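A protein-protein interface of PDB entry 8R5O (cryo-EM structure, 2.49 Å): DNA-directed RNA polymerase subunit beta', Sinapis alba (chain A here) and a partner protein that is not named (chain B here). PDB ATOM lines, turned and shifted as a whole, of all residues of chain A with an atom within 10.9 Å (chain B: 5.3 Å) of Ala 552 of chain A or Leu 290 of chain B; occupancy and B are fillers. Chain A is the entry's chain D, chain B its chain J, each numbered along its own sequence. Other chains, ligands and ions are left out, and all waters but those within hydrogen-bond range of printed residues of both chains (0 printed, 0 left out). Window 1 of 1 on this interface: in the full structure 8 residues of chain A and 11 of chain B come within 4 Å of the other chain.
The guanidinium group (NH1) of Arg 287 of chain B lies within hydrogen-bond range of the backbone carbonyl oxygen (O) of Ile 550 of chain A, at 2.7 Å.
NH2 of Arg 287 of chain B lies within hydrogen-bond range of O of Arg 554 of chain A (3.1 Å).
The guanidinium group (NH1) of Arg 287 of chain B is in hydrogen-bond range of the backbone carbonyl oxygen (O) of Asn 553 of chain A, at 3.2 Å.
A ring nitrogen (NE2) of His 289 of chain B lies within hydrogen-bond range of the backbone carbonyl oxygen (O) of Cys 551 of chain A, at 2.6 Å.
NE of Arg 554 of chain A lies within salt-bridge range of OE1 of Glu 294 of chain B, 3.6 Å away.
The guanidinium group (NH1) of Arg 554 of chain A lies close to the side-chain hydroxyl (OH) of Tyr 555 of chain A (3.4 Å).
Among the printed residues, pairs that only touch across the chains: Ile 550 of chain A with Leu 290 of chain B (3.3 Å), Arg 554 of chain A with Phe 291 of chain B (3.4 Å), Arg 547 of chain A with His 289 of chain B (3.4 Å), Ala 552 of chain A with Leu 290 of chain B (3.6 Å), Arg 554 of chain A with Leu 290 of chain B (3.7 Å), Asn 553 of chain A with Leu 290 of chain B (3.7 Å) and Cys 551 of chain A with Leu 290 of chain B (3.7 Å).
Of the printed residues of chain B, Arg 547 of chain A touches His 289 (3.4 Å).
Printed residues of chain B within 4 Å of Ile 550 of chain A: Arg 287 (2.7 Å) and Leu 290 (3.3 Å).
Of the printed residues of chain B, Ala 552 of chain A touches Leu 290 (3.6 Å).
Of the printed residues of chain B, Arg 554 of chain A touches Arg 287 (3.1 Å), Leu 290 (3.7 Å), Phe 291 (3.4 Å) and Glu 294 (3.3 Å).
Glu 578 of chain A touches none of the printed residues of chain B.
Asp 599 of chain A touches none of the printed residues of chain B.
Of chain A, only Ile 550 (2.7 Å), Asn 553 (3.2 Å) and Arg 554 (3.1 Å) come within 4 Å of Arg 287 of chain B.
His 289 of chain B touches just these residues of chain A: Arg 547 (3.4 Å) and Cys 551 (2.6 Å).
Printed residues of chain A within 4 Å of Leu 290 of chain B: Ile 550, Cys 551, Ala 552, Asn 553 and Arg 554.
Phe 291 of chain B touches just one residue of chain A: Arg 554 (3.4 Å).
No residue of chain A comes within 4 Å of Glu 293 of chain B.
The nearest residue of chain B that does not touch Ala 552 of chain A is His 289 of chain B (4.8 Å).
The nearest residue of chain A that does not touch Leu 290 of chain B is Gly 549 of chain A (5.9 Å).
Printed residues of chain B that touch a printed residue of chain A: Arg 287, His 289, Leu 290, Phe 291 and Glu 294.
Hydrophobic or aromatic side chains of chain B that line the printed part of chain A: His 289, Leu 290 and Phe 291.
Hydrophobic or aromatic side chains of chain A within 4 Å of the printed part of chain B: Ile 550.
Along chain A the printed residues that touch a printed residue of chain B span positions 547 to 554.
Among the printed residues, 12 pairs touch across the chains.
Among the printed residues, Asp or Glu carboxylates within 4 Å of a Lys or Arg side-chain nitrogen of the other chain: Arg 554 of chain A with Glu 294 of chain B (3.6 Å).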
ATOM      1  N   GLY A 545      37.365 -17.870  12.149  1.00  0.00           N
ATOM      2  CA  GLY A 545      36.922 -16.695  11.429  1.00  0.00           C
ATOM      3  C   GLY A 545      35.432 -16.627  11.177  1.00  0.00           C
ATOM      4  O   GLY A 545      34.629 -17.068  12.003  1.00  0.00           O
ATOM      5  N   THR A 546      35.053 -16.069  10.035  1.00  0.00           N
ATOM      6  CA  THR A 546      33.652 -15.880   9.709  1.00  0.00           C
ATOM      7  C   THR A 546      33.040 -17.168   9.164  1.00  0.00           C
ATOM      8  O   THR A 546      33.722 -18.027   8.601  1.00  0.00           O
ATOM      9  CB  THR A 546      33.485 -14.753   8.689  1.00  0.00           C
ATOM     10  OG1 THR A 546      32.108 -14.641   8.319  1.00  0.00           O
ATOM     11  CG2 THR A 546      34.321 -15.026   7.448  1.00  0.00           C
ATOM     12  N   ARG A 547      31.730 -17.298   9.354  1.00  0.00           N
ATOM     13  CA  ARG A 547      30.983 -18.368   8.715  1.00  0.00           C
ATOM     14  C   ARG A 547      30.952 -18.156   7.206  1.00  0.00           C
ATOM     15  O   ARG A 547      30.949 -17.024   6.715  1.00  0.00           O
ATOM     16  CB  ARG A 547      29.565 -18.438   9.284  1.00  0.00           C
ATOM     17  CG  ARG A 547      29.433 -19.433  10.420  1.00  0.00           C
ATOM     18  CD  ARG A 547      28.292 -19.101  11.362  1.00  0.00           C
ATOM     19  NE  ARG A 547      27.988 -20.231  12.232  1.00  0.00           N
ATOM     20  CZ  ARG A 547      27.275 -20.156  13.347  1.00  0.00           C
ATOM     21  NH1 ARG A 547      26.802 -19.003  13.789  1.00  0.00           N
ATOM     22  NH2 ARG A 547      27.036 -21.266  14.038  1.00  0.00           N
ATOM     23  N   ARG A 548      30.947 -19.262   6.465  1.00  0.00           N
ATOM     24  CA  ARG A 548      31.132 -19.223   5.022  1.00  0.00           C
ATOM     25  C   ARG A 548      30.051 -20.021   4.307  1.00  0.00           C
ATOM     26  O   ARG A 548      29.537 -21.013   4.829  1.00  0.00           O
ATOM     27  CB  ARG A 548      32.511 -19.768   4.625  1.00  0.00           C
ATOM     28  CG  ARG A 548      33.670 -18.982   5.199  1.00  0.00           C
ATOM     29  CD  ARG A 548      35.003 -19.518   4.721  1.00  0.00           C
ATOM     30  NE  ARG A 548      36.111 -18.745   5.267  1.00  0.00           N
ATOM     31  CZ  ARG A 548      36.585 -17.630   4.727  1.00  0.00           C
ATOM     32  NH1 ARG A 548      36.079 -17.135   3.610  1.00  0.00           N
ATOM     33  NH2 ARG A 548      37.590 -16.997   5.323  1.00  0.00           N
ATOM     34  N   GLY A 549      29.719 -19.569   3.102  1.00  0.00           N
ATOM     35  CA  GLY A 549      28.858 -20.345   2.220  1.00  0.00           C
ATOM     36  C   GLY A 549      27.444 -20.472   2.747  1.00  0.00           C
ATOM     37  O   GLY A 549      26.812 -19.488   3.147  1.00  0.00           O
ATOM     38  N   ILE A 550      26.930 -21.705   2.743  1.00  0.00           N
ATOM     39  CA  ILE A 550      25.563 -21.961   3.181  1.00  0.00           C
ATOM     40  C   ILE A 550      25.368 -21.741   4.670  1.00  0.00           C
ATOM     41  O   ILE A 550      24.225 -21.658   5.130  1.00  0.00           O
ATOM     42  CB  ILE A 550      25.129 -23.394   2.817  1.00  0.00           C
ATOM     43  CG1 ILE A 550      26.036 -24.411   3.508  1.00  0.00           C
ATOM     44  CG2 ILE A 550      25.143 -23.588   1.309  1.00  0.00           C
ATOM     45  CD1 ILE A 550      25.608 -25.834   3.313  1.00  0.00           C
ATOM     46  N   CYS A 551      26.450 -21.648   5.440  1.00  0.00           N
ATOM     47  CA  CYS A 551      26.362 -21.295   6.847  1.00  0.00           C
ATOM     48  C   CYS A 551      26.355 -19.790   7.076  1.00  0.00           C
ATOM     49  O   CYS A 551      26.128 -19.353   8.209  1.00  0.00           O
ATOM     50  CB  CYS A 551      27.520 -21.927   7.625  1.00  0.00           C
ATOM     51  SG  CYS A 551      27.549 -23.730   7.573  1.00  0.00           S
ATOM     52  N   ALA A 552      26.596 -18.994   6.037  1.00  0.00           N
ATOM     53  CA  ALA A 552      26.590 -17.542   6.135  1.00  0.00           C
ATOM     54  C   ALA A 552      25.388 -16.888   5.475  1.00  0.00           C
ATOM     55  O   ALA A 552      24.965 -15.820   5.915  1.00  0.00           O
ATOM     56  CB  ALA A 552      27.867 -16.960   5.515  1.00  0.00           C
ATOM     57  N   ASN A 553      24.828 -17.499   4.433  1.00  0.00           N
ATOM     58  CA  ASN A 553      23.691 -16.942   3.714  1.00  0.00           C
ATOM     59  C   ASN A 553      22.637 -18.020   3.529  1.00  0.00           C
ATOM     60  O   ASN A 553      22.961 -19.146   3.142  1.00  0.00           O
ATOM     61  CB  ASN A 553      24.113 -16.379   2.352  1.00  0.00           C
ATOM     62  CG  ASN A 553      25.114 -15.251   2.474  1.00  0.00           C
ATOM     63  OD1 ASN A 553      24.754 -14.122   2.803  1.00  0.00           O
ATOM     64  ND2 ASN A 553      26.377 -15.550   2.207  1.00  0.00           N
ATOM     65  N   ARG A 554      21.379 -17.677   3.812  1.00  0.00           N
ATOM     66  CA  ARG A 554      20.290 -18.620   3.585  1.00  0.00           C
ATOM     67  C   ARG A 554      20.126 -18.918   2.101  1.00  0.00           C
ATOM     68  O   ARG A 554      19.906 -20.070   1.711  1.00  0.00           O
ATOM     69  CB  ARG A 554      18.988 -18.070   4.167  1.00  0.00           C
ATOM     70  CG  ARG A 554      17.851 -19.081   4.234  1.00  0.00           C
ATOM     71  CD  ARG A 554      16.505 -18.382   4.194  1.00  0.00           C
ATOM     72  NE  ARG A 554      15.379 -19.263   4.491  1.00  0.00           N
ATOM     73  CZ  ARG A 554      14.904 -20.186   3.668  1.00  0.00           C
ATOM     74  NH1 ARG A 554      15.480 -20.442   2.506  1.00  0.00           N
ATOM     75  NH2 ARG A 554      13.823 -20.875   4.022  1.00  0.00           N
ATOM     76  N   TYR A 555      20.241 -17.899   1.259  1.00  0.00           N
ATOM     77  CA  TYR A 555      20.058 -18.041  -0.175  1.00  0.00           C
ATOM     78  C   TYR A 555      21.381 -17.851  -0.904  1.00  0.00           C
ATOM     79  O   TYR A 555      22.295 -17.185  -0.411  1.00  0.00           O
ATOM     80  CB  TYR A 555      19.033 -17.035  -0.706  1.00  0.00           C
ATOM     81  CG  TYR A 555      17.659 -17.200  -0.107  1.00  0.00           C
ATOM     82  CD1 TYR A 555      16.865 -18.288  -0.434  1.00  0.00           C
ATOM     83  CD2 TYR A 555      17.153 -16.265   0.785  1.00  0.00           C
ATOM     84  CE1 TYR A 555      15.610 -18.443   0.111  1.00  0.00           C
ATOM     85  CE2 TYR A 555      15.899 -16.412   1.335  1.00  0.00           C
ATOM     86  CZ  TYR A 555      15.131 -17.503   0.997  1.00  0.00           C
ATOM     87  OH  TYR A 555      13.880 -17.650   1.546  1.00  0.00           O
ATOM     88  N   ASN A 556      21.471 -18.457  -2.078  1.00  0.00           N
ATOM     89  CA  ASN A 556      22.614 -18.277  -2.956  1.00  0.00           C
ATOM     90  C   ASN A 556      22.683 -16.824  -3.412  1.00  0.00           C
ATOM     91  O   ASN A 556      21.707 -16.317  -3.983  1.00  0.00           O
ATOM     92  CB  ASN A 556      22.485 -19.208  -4.160  1.00  0.00           C
ATOM     93  CG  ASN A 556      23.747 -19.272  -4.997  1.00  0.00           C
ATOM     94  OD1 ASN A 556      24.670 -18.480  -4.822  1.00  0.00           O
ATOM     95  ND2 ASN A 556      23.789 -20.221  -5.924  1.00  0.00           N
ATOM     96  N   PRO A 557      23.795 -16.122  -3.189  1.00  0.00           N
ATOM     97  CA  PRO A 557      23.906 -14.746  -3.690  1.00  0.00           C
ATOM     98  C   PRO A 557      24.097 -14.690  -5.198  1.00  0.00           C
ATOM     99  O   PRO A 557      25.051 -14.071  -5.679  1.00  0.00           O
ATOM    100  CB  PRO A 557      25.137 -14.198  -2.953  1.00  0.00           C
ATOM    101  CG  PRO A 557      25.404 -15.168  -1.838  1.00  0.00           C
ATOM    102  CD  PRO A 557      24.930 -16.489  -2.329  1.00  0.00           C
ATOM    103  N   GLU A 578      29.898  -5.250   3.510  1.00  0.00           N
ATOM    104  CA  GLU A 578      30.830  -5.423   4.617  1.00  0.00           C
ATOM    105  C   GLU A 578      31.665  -4.164   4.826  1.00  0.00           C
ATOM    106  O   GLU A 578      32.033  -3.492   3.867  1.00  0.00           O
ATOM    107  CB  GLU A 578      31.725  -6.639   4.372  1.00  0.00           C
ATOM    108  CG  GLU A 578      30.961  -7.952   4.389  1.00  0.00           C
ATOM    109  CD  GLU A 578      31.786  -9.127   3.908  1.00  0.00           C
ATOM    110  OE1 GLU A 578      32.930  -8.913   3.463  1.00  0.00           O
ATOM    111  OE2 GLU A 578      31.284 -10.268   3.974  1.00  0.00           O
ATOM    112  N   ASP A 599      33.669 -12.259  14.939  1.00  0.00           N
ATOM    113  CA  ASP A 599      33.859 -13.079  13.750  1.00  0.00           C
ATOM    114  C   ASP A 599      33.099 -12.538  12.543  1.00  0.00           C
ATOM    115  O   ASP A 599      32.914 -13.260  11.561  1.00  0.00           O
ATOM    116  CB  ASP A 599      33.445 -14.523  14.030  1.00  0.00           C
ATOM    117  CG  ASP A 599      31.982 -14.647  14.397  1.00  0.00           C
ATOM    118  OD1 ASP A 599      31.440 -13.706  15.012  1.00  0.00           O
ATOM    119  OD2 ASP A 599      31.372 -15.683  14.064  1.00  0.00           O
ATOM    120  N   SER A 600      32.652 -11.291  12.592  1.00  0.00           N
ATOM    121  CA  SER A 600      31.998 -10.696  11.433  1.00  0.00           C
ATOM    122  C   SER A 600      33.044 -10.286  10.401  1.00  0.00           C
ATOM    123  O   SER A 600      34.034  -9.641  10.758  1.00  0.00           O
ATOM    124  CB  SER A 600      31.158  -9.492  11.845  1.00  0.00           C
ATOM    125  OG  SER A 600      31.934  -8.540  12.545  1.00  0.00           O
ATOM    126  N   PRO A 601      32.870 -10.646   9.131  1.00  0.00           N
ATOM    127  CA  PRO A 601      33.897 -10.339   8.131  1.00  0.00           C
ATOM    128  C   PRO A 601      34.022  -8.846   7.873  1.00  0.00           C
ATOM    129  O   PRO A 601      33.058  -8.085   7.981  1.00  0.00           O
ATOM    130  CB  PRO A 601      33.406 -11.079   6.882  1.00  0.00           C
ATOM    131  CG  PRO A 601      31.938 -11.188   7.064  1.00  0.00           C
ATOM    132  CD  PRO A 601      31.707 -11.330   8.542  1.00  0.00           C
ATOM    133  N   ARG A 653      40.383  -9.511   3.522  1.00  0.00           N
ATOM    134  CA  ARG A 653      39.109  -9.897   4.115  1.00  0.00           C
ATOM    135  C   ARG A 653      39.405 -10.758   5.337  1.00  0.00           C
ATOM    136  O   ARG A 653      39.843 -11.904   5.207  1.00  0.00           O
ATOM    137  CB  ARG A 653      38.239 -10.635   3.102  1.00  0.00           C
ATOM    138  CG  ARG A 653      36.823 -10.889   3.576  1.00  0.00           C
ATOM    139  CD  ARG A 653      35.933 -11.341   2.434  1.00  0.00           C
ATOM    140  NE  ARG A 653      34.556 -11.552   2.865  1.00  0.00           N
ATOM    141  CZ  ARG A 653      34.056 -12.722   3.238  1.00  0.00           C
ATOM    142  NH1 ARG A 653      34.793 -13.820   3.239  1.00  0.00           N
ATOM    143  NH2 ARG A 653      32.785 -12.791   3.619  1.00  0.00           N
ATOM    144  N   ARG B 287      22.386 -24.713   9.737  1.00  0.00           N
ATOM    145  CA  ARG B 287      21.954 -23.375   9.345  1.00  0.00           C
ATOM    146  C   ARG B 287      20.896 -22.793  10.279  1.00  0.00           C
ATOM    147  O   ARG B 287      20.170 -21.879   9.884  1.00  0.00           O
ATOM    148  CB  ARG B 287      21.437 -23.380   7.904  1.00  0.00           C
ATOM    149  CG  ARG B 287      21.834 -24.607   7.103  1.00  0.00           C
ATOM    150  CD  ARG B 287      21.951 -24.337   5.608  1.00  0.00           C
ATOM    151  NE  ARG B 287      20.729 -23.805   5.013  1.00  0.00           N
ATOM    152  CZ  ARG B 287      20.671 -22.694   4.291  1.00  0.00           C
ATOM    153  NH1 ARG B 287      21.750 -21.974   4.041  1.00  0.00           N
ATOM    154  NH2 ARG B 287      19.500 -22.304   3.796  1.00  0.00           N
ATOM    155  N   ARG B 288      20.801 -23.293  11.514  1.00  0.00           N
ATOM    156  CA  ARG B 288      19.748 -22.833  12.416  1.00  0.00           C
ATOM    157  C   ARG B 288      19.917 -21.368  12.798  1.00  0.00           C
ATOM    158  O   ARG B 288      18.924 -20.683  13.068  1.00  0.00           O
ATOM    159  CB  ARG B 288      19.712 -23.699  13.676  1.00  0.00           C
ATOM    160  CG  ARG B 288      20.972 -23.618  14.513  1.00  0.00           C
ATOM    161  CD  ARG B 288      20.993 -24.660  15.609  1.00  0.00           C
ATOM    162  NE  ARG B 288      22.280 -24.675  16.292  1.00  0.00           N
ATOM    163  CZ  ARG B 288      22.701 -25.652  17.082  1.00  0.00           C
ATOM    164  NH1 ARG B 288      21.960 -26.725  17.310  1.00  0.00           N
ATOM    165  NH2 ARG B 288      23.897 -25.553  17.654  1.00  0.00           N
ATOM    166  N   HIS B 289      21.154 -20.871  12.833  1.00  0.00           N
ATOM    167  CA  HIS B 289      21.386 -19.483  13.214  1.00  0.00           C
ATOM    168  C   HIS B 289      20.855 -18.515  12.164  1.00  0.00           C
ATOM    169  O   HIS B 289      20.464 -17.393  12.500  1.00  0.00           O
ATOM    170  CB  HIS B 289      22.877 -19.249  13.451  1.00  0.00           C
ATOM    171  CG  HIS B 289      23.731 -19.592  12.270  1.00  0.00           C
ATOM    172  ND1 HIS B 289      24.011 -20.891  11.907  1.00  0.00           N
ATOM    173  CD2 HIS B 289      24.359 -18.805  11.367  1.00  0.00           C
ATOM    174  CE1 HIS B 289      24.776 -20.889  10.832  1.00  0.00           C
ATOM    175  NE2 HIS B 289      25.002 -19.636  10.484  1.00  0.00           N
ATOM    176  N   LEU B 290      20.841 -18.924  10.895  1.00  0.00           N
ATOM    177  CA  LEU B 290      20.300 -18.068   9.845  1.00  0.00           C
ATOM    178  C   LEU B 290      18.803 -17.846  10.022  1.00  0.00           C
ATOM    179  O   LEU B 290      18.319 -16.717   9.891  1.00  0.00           O
ATOM    180  CB  LEU B 290      20.592 -18.675   8.476  1.00  0.00           C
ATOM    181  CG  LEU B 290      22.065 -18.922   8.150  1.00  0.00           C
ATOM    182  CD1 LEU B 290      22.195 -19.653   6.828  1.00  0.00           C
ATOM    183  CD2 LEU B 290      22.834 -17.612   8.122  1.00  0.00           C
ATOM    184  N   PHE B 291      18.055 -18.909  10.327  1.00  0.00           N
ATOM    185  CA  PHE B 291      16.607 -18.785  10.453  1.00  0.00           C
ATOM    186  C   PHE B 291      16.223 -17.990  11.694  1.00  0.00           C
ATOM    187  O   PHE B 291      15.252 -17.226  11.671  1.00  0.00           O
ATOM    188  CB  PHE B 291      15.962 -20.170  10.474  1.00  0.00           C
ATOM    189  CG  PHE B 291      16.311 -21.014   9.284  1.00  0.00           C
ATOM    190  CD1 PHE B 291      15.820 -20.700   8.030  1.00  0.00           C
ATOM    191  CD2 PHE B 291      17.128 -22.122   9.419  1.00  0.00           C
ATOM    192  CE1 PHE B 291      16.141 -21.470   6.934  1.00  0.00           C
ATOM    193  CE2 PHE B 291      17.452 -22.896   8.326  1.00  0.00           C
ATOM    194  CZ  PHE B 291      16.958 -22.569   7.081  1.00  0.00           C
ATOM    195  N   LYS B 292      16.968 -18.157  12.788  1.00  0.00           N
ATOM    196  CA  LYS B 292      16.706 -17.358  13.979  1.00  0.00           C
ATOM    197  C   LYS B 292      16.945 -15.879  13.710  1.00  0.00           C
ATOM    198  O   LYS B 292      16.180 -15.024  14.172  1.00  0.00           O
ATOM    199  CB  LYS B 292      17.573 -17.836  15.142  1.00  0.00           C
ATOM    200  CG  LYS B 292      17.351 -17.042  16.416  1.00  0.00           C
ATOM    201  CD  LYS B 292      18.334 -17.423  17.505  1.00  0.00           C
ATOM    202  CE  LYS B 292      18.166 -16.524  18.718  1.00  0.00           C
ATOM    203  NZ  LYS B 292      19.113 -16.864  19.814  1.00  0.00           N
ATOM    204  N   GLU B 293      18.001 -15.557  12.961  1.00  0.00           N
ATOM    205  CA  GLU B 293      18.281 -14.162  12.639  1.00  0.00           C
ATOM    206  C   GLU B 293      17.152 -13.548  11.820  1.00  0.00           C
ATOM    207  O   GLU B 293      16.816 -12.373  12.001  1.00  0.00           O
ATOM    208  CB  GLU B 293      19.613 -14.053  11.897  1.00  0.00           C
ATOM    209  CG  GLU B 293      19.981 -12.637  11.495  1.00  0.00           C
ATOM    210  CD  GLU B 293      19.997 -11.680  12.673  1.00  0.00           C
ATOM    211  OE1 GLU B 293      20.426 -12.090  13.773  1.00  0.00           O
ATOM    212  OE2 GLU B 293      19.574 -10.518  12.503  1.00  0.00           O
ATOM    213  N   GLU B 294      16.552 -14.330  10.920  1.00  0.00           N
ATOM    214  CA  GLU B 294      15.405 -13.841  10.162  1.00  0.00           C
ATOM    215  C   GLU B 294      14.237 -13.500  11.079  1.00  0.00           C
ATOM    216  O   GLU B 294      13.588 -12.463  10.907  1.00  0.00           O
ATOM    217  CB  GLU B 294      14.975 -14.876   9.121  1.00  0.00           C
ATOM    218  CG  GLU B 294      15.867 -14.943   7.897  1.00  0.00           C
ATOM    219  CD  GLU B 294      15.382 -15.954   6.873  1.00  0.00           C
ATOM    220  OE1 GLU B 294      14.973 -17.064   7.274  1.00  0.00           O
ATOM    221  OE2 GLU B 294      15.404 -15.634   5.666  1.00  0.00           O
